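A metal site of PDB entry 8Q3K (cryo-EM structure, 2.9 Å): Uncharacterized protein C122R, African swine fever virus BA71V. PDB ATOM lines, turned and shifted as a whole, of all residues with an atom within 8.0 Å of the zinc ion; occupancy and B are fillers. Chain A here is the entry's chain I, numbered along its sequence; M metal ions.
The zinc ion is bound by the side-chain sulfur of Cys 26, the side-chain sulfur of Cys 7, the side-chain sulfur of Cys 24 and the side-chain sulfur of Cys 4. The zinc ion has four donor atoms within binding distance.
Within 4 Å of the zinc ion: Cys 4, Cys 7, Cys 24 and Cys 26. Along chain A the residues within 4 Å of the zinc ion span positions 4 to 26. The nearest printed residue that does not touch the zinc ion is Ser 9 (4.2 Å).
The backbone NH of Cys 4 sits close to the side-chain sulfur of Met 11 (3.7 Å).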
ATOM      1  N   LYS A   2       2.821  10.356  23.745  1.00  0.00           N
ATOM      2  CA  LYS A   2       3.803  11.420  23.724  1.00  0.00           C
ATOM      3  C   LYS A   2       3.116  12.737  23.396  1.00  0.00           C
ATOM      4  O   LYS A   2       2.281  12.789  22.487  1.00  0.00           O
ATOM      5  CB  LYS A   2       4.913  11.142  22.707  1.00  0.00           C
ATOM      6  CG  LYS A   2       6.161  10.486  23.279  1.00  0.00           C
ATOM      7  CD  LYS A   2       7.410  10.993  22.597  1.00  0.00           C
ATOM      8  CE  LYS A   2       8.614  10.117  22.891  1.00  0.00           C
ATOM      9  NZ  LYS A   2       8.912  10.052  24.356  1.00  0.00           N
ATOM     10  N   ILE A   3       3.469  13.786  24.127  1.00  0.00           N
ATOM     11  CA  ILE A   3       2.940  15.133  23.900  1.00  0.00           C
ATOM     12  C   ILE A   3       4.124  16.066  23.752  1.00  0.00           C
ATOM     13  O   ILE A   3       4.929  16.223  24.677  1.00  0.00           O
ATOM     14  CB  ILE A   3       2.017  15.577  25.042  1.00  0.00           C
ATOM     15  CG1 ILE A   3       2.574  15.128  26.390  1.00  0.00           C
ATOM     16  CG2 ILE A   3       0.609  15.041  24.828  1.00  0.00           C
ATOM     17  CD1 ILE A   3       1.795  15.642  27.576  1.00  0.00           C
ATOM     18  N   CYS A   4       4.221  16.712  22.588  1.00  0.00           N
ATOM     19  CA  CYS A   4       5.327  17.637  22.349  1.00  0.00           C
ATOM     20  C   CYS A   4       5.243  18.806  23.316  1.00  0.00           C
ATOM     21  O   CYS A   4       4.174  19.388  23.539  1.00  0.00           O
ATOM     22  CB  CYS A   4       5.298  18.135  20.903  1.00  0.00           C
ATOM     23  SG  CYS A   4       3.656  18.400  20.225  1.00  0.00           S
ATOM     24  N   LYS A   5       6.392  19.159  23.897  1.00  0.00           N
ATOM     25  CA  LYS A   5       6.432  20.227  24.888  1.00  0.00           C
ATOM     26  C   LYS A   5       5.985  21.561  24.299  1.00  0.00           C
ATOM     27  O   LYS A   5       5.483  22.430  25.028  1.00  0.00           O
ATOM     28  CB  LYS A   5       7.847  20.351  25.465  1.00  0.00           C
ATOM     29  CG  LYS A   5       8.431  19.059  26.077  1.00  0.00           C
ATOM     30  CD  LYS A   5       7.445  18.175  26.865  1.00  0.00           C
ATOM     31  CE  LYS A   5       6.620  18.936  27.892  1.00  0.00           C
ATOM     32  NZ  LYS A   5       7.456  19.848  28.727  1.00  0.00           N
ATOM     33  N   ALA A   6       6.153  21.751  22.987  1.00  0.00           N
ATOM     34  CA  ALA A   6       5.688  22.982  22.353  1.00  0.00           C
ATOM     35  C   ALA A   6       4.173  23.113  22.474  1.00  0.00           C
ATOM     36  O   ALA A   6       3.660  24.198  22.798  1.00  0.00           O
ATOM     37  CB  ALA A   6       6.095  23.014  20.881  1.00  0.00           C
ATOM     38  N   CYS A   7       3.442  22.035  22.225  1.00  0.00           N
ATOM     39  CA  CYS A   7       1.993  22.039  22.339  1.00  0.00           C
ATOM     40  C   CYS A   7       1.534  20.648  22.762  1.00  0.00           C
ATOM     41  O   CYS A   7       1.991  19.650  22.212  1.00  0.00           O
ATOM     42  CB  CYS A   7       1.326  22.447  21.021  1.00  0.00           C
ATOM     43  SG  CYS A   7       1.012  21.090  19.860  1.00  0.00           S
ATOM     44  N   SER A   8       0.632  20.601  23.738  1.00  0.00           N
ATOM     45  CA  SER A   8       0.092  19.333  24.201  1.00  0.00           C
ATOM     46  C   SER A   8      -0.773  18.724  23.110  1.00  0.00           C
ATOM     47  O   SER A   8      -1.909  19.168  22.895  1.00  0.00           O
ATOM     48  CB  SER A   8      -0.700  19.529  25.488  1.00  0.00           C
ATOM     49  OG  SER A   8       0.166  19.862  26.569  1.00  0.00           O
ATOM     50  N   SER A   9      -0.255  17.719  22.422  1.00  0.00           N
ATOM     51  CA  SER A   9      -0.978  17.067  21.343  1.00  0.00           C
ATOM     52  C   SER A   9      -0.345  15.708  21.090  1.00  0.00           C
ATOM     53  O   SER A   9       0.854  15.507  21.315  1.00  0.00           O
ATOM     54  CB  SER A   9      -0.958  17.908  20.063  1.00  0.00           C
ATOM     55  OG  SER A   9      -1.661  17.260  19.014  1.00  0.00           O
ATOM     56  N   CYS A  10      -1.159  14.773  20.616  1.00  0.00           N
ATOM     57  CA  CYS A  10      -0.682  13.419  20.354  1.00  0.00           C
ATOM     58  C   CYS A  10       0.398  13.436  19.287  1.00  0.00           C
ATOM     59  O   CYS A  10       0.254  14.090  18.245  1.00  0.00           O
ATOM     60  CB  CYS A  10      -1.842  12.528  19.916  1.00  0.00           C
ATOM     61  SG  CYS A  10      -3.272  12.549  21.032  1.00  0.00           S
ATOM     62  N   MET A  11       1.491  12.733  19.549  1.00  0.00           N
ATOM     63  CA  MET A  11       2.597  12.595  18.596  1.00  0.00           C
ATOM     64  C   MET A  11       2.310  11.376  17.724  1.00  0.00           C
ATOM     65  O   MET A  11       2.325  10.244  18.215  1.00  0.00           O
ATOM     66  CB  MET A  11       3.924  12.451  19.332  1.00  0.00           C
ATOM     67  CG  MET A  11       4.324  13.652  20.176  1.00  0.00           C
ATOM     68  SD  MET A  11       4.594  15.162  19.230  1.00  0.00           S
ATOM     69  CE  MET A  11       6.090  14.740  18.332  1.00  0.00           C
ATOM     70  N   ARG A  23       6.257  12.771  15.592  1.00  0.00           N
ATOM     71  CA  ARG A  23       5.944  14.062  14.984  1.00  0.00           C
ATOM     72  C   ARG A  23       4.568  14.530  15.421  1.00  0.00           C
ATOM     73  O   ARG A  23       3.699  13.732  15.786  1.00  0.00           O
ATOM     74  CB  ARG A  23       6.002  13.996  13.442  1.00  0.00           C
ATOM     75  CG  ARG A  23       7.198  13.218  12.894  1.00  0.00           C
ATOM     76  CD  ARG A  23       7.171  13.156  11.374  1.00  0.00           C
ATOM     77  NE  ARG A  23       7.225  14.477  10.765  1.00  0.00           N
ATOM     78  CZ  ARG A  23       7.204  14.704   9.466  1.00  0.00           C
ATOM     79  NH1 ARG A  23       7.126  13.715   8.585  1.00  0.00           N
ATOM     80  NH2 ARG A  23       7.267  15.963   9.020  1.00  0.00           N
ATOM     81  N   CYS A  24       4.382  15.853  15.376  1.00  0.00           N
ATOM     82  CA  CYS A  24       3.085  16.484  15.608  1.00  0.00           C
ATOM     83  C   CYS A  24       2.751  17.401  14.437  1.00  0.00           C
ATOM     84  O   CYS A  24       3.534  17.586  13.507  1.00  0.00           O
ATOM     85  CB  CYS A  24       3.081  17.297  16.914  1.00  0.00           C
ATOM     86  SG  CYS A  24       1.643  18.378  17.105  1.00  0.00           S
ATOM     87  N   SER A  25       1.544  17.967  14.499  1.00  0.00           N
ATOM     88  CA  SER A  25       1.141  18.948  13.488  1.00  0.00           C
ATOM     89  C   SER A  25       1.997  20.208  13.566  1.00  0.00           C
ATOM     90  O   SER A  25       2.148  20.910  12.561  1.00  0.00           O
ATOM     91  CB  SER A  25      -0.332  19.296  13.652  1.00  0.00           C
ATOM     92  OG  SER A  25      -0.752  20.227  12.671  1.00  0.00           O
ATOM     93  N   CYS A  26       2.549  20.503  14.734  1.00  0.00           N
ATOM     94  CA  CYS A  26       3.370  21.687  14.929  1.00  0.00           C
ATOM     95  C   CYS A  26       4.853  21.441  14.660  1.00  0.00           C
ATOM     96  O   CYS A  26       5.627  22.411  14.649  1.00  0.00           O
ATOM     97  CB  CYS A  26       3.211  22.208  16.362  1.00  0.00           C
ATOM     98  SG  CYS A  26       4.061  21.217  17.622  1.00  0.00           S
ATOM     99  N   GLY A  27       5.265  20.195  14.444  1.00  0.00           N
ATOM    100  CA  GLY A  27       6.670  19.890  14.243  1.00  0.00           C
ATOM    101  C   GLY A  27       7.368  19.500  15.522  1.00  0.00           C
ATOM    102  O   GLY A  27       6.813  18.762  16.338  1.00  0.00           O
ATOM    103  N   GLU A  28       8.594  19.990  15.716  1.00  0.00           N
ATOM    104  CA  GLU A  28       9.372  19.738  16.928  1.00  0.00           C
ATOM    105  C   GLU A  28       9.663  18.255  17.118  1.00  0.00           C
ATOM    106  O   GLU A  28      10.115  17.822  18.185  1.00  0.00           O
ATOM    107  CB  GLU A  28       8.651  20.348  18.150  1.00  0.00           C
ATOM    108  CG  GLU A  28       9.048  19.871  19.546  1.00  0.00           C
ATOM    109  CD  GLU A  28       8.340  18.588  19.966  1.00  0.00           C
ATOM    110  OE1 GLU A  28       7.627  18.005  19.128  1.00  0.00           O
ATOM    111  OE2 GLU A  28       8.497  18.184  21.136  1.00  0.00           O
ATOM    112  N   SER A  29       9.497  17.469  16.043  1.00  0.00           N
ATOM    113  CA  SER A  29       9.554  16.012  16.123  1.00  0.00           C
ATOM    114  C   SER A  29      10.705  15.540  16.991  1.00  0.00           C
ATOM    115  O   SER A  29      11.805  16.096  16.959  1.00  0.00           O
ATOM    116  CB  SER A  29       9.694  15.437  14.711  1.00  0.00           C
ATOM    117  OG  SER A  29      10.278  14.141  14.745  1.00  0.00           O
HETATM  118 ZN    ZN M   1       2.568  19.801  18.706  1.00  0.00          ZN
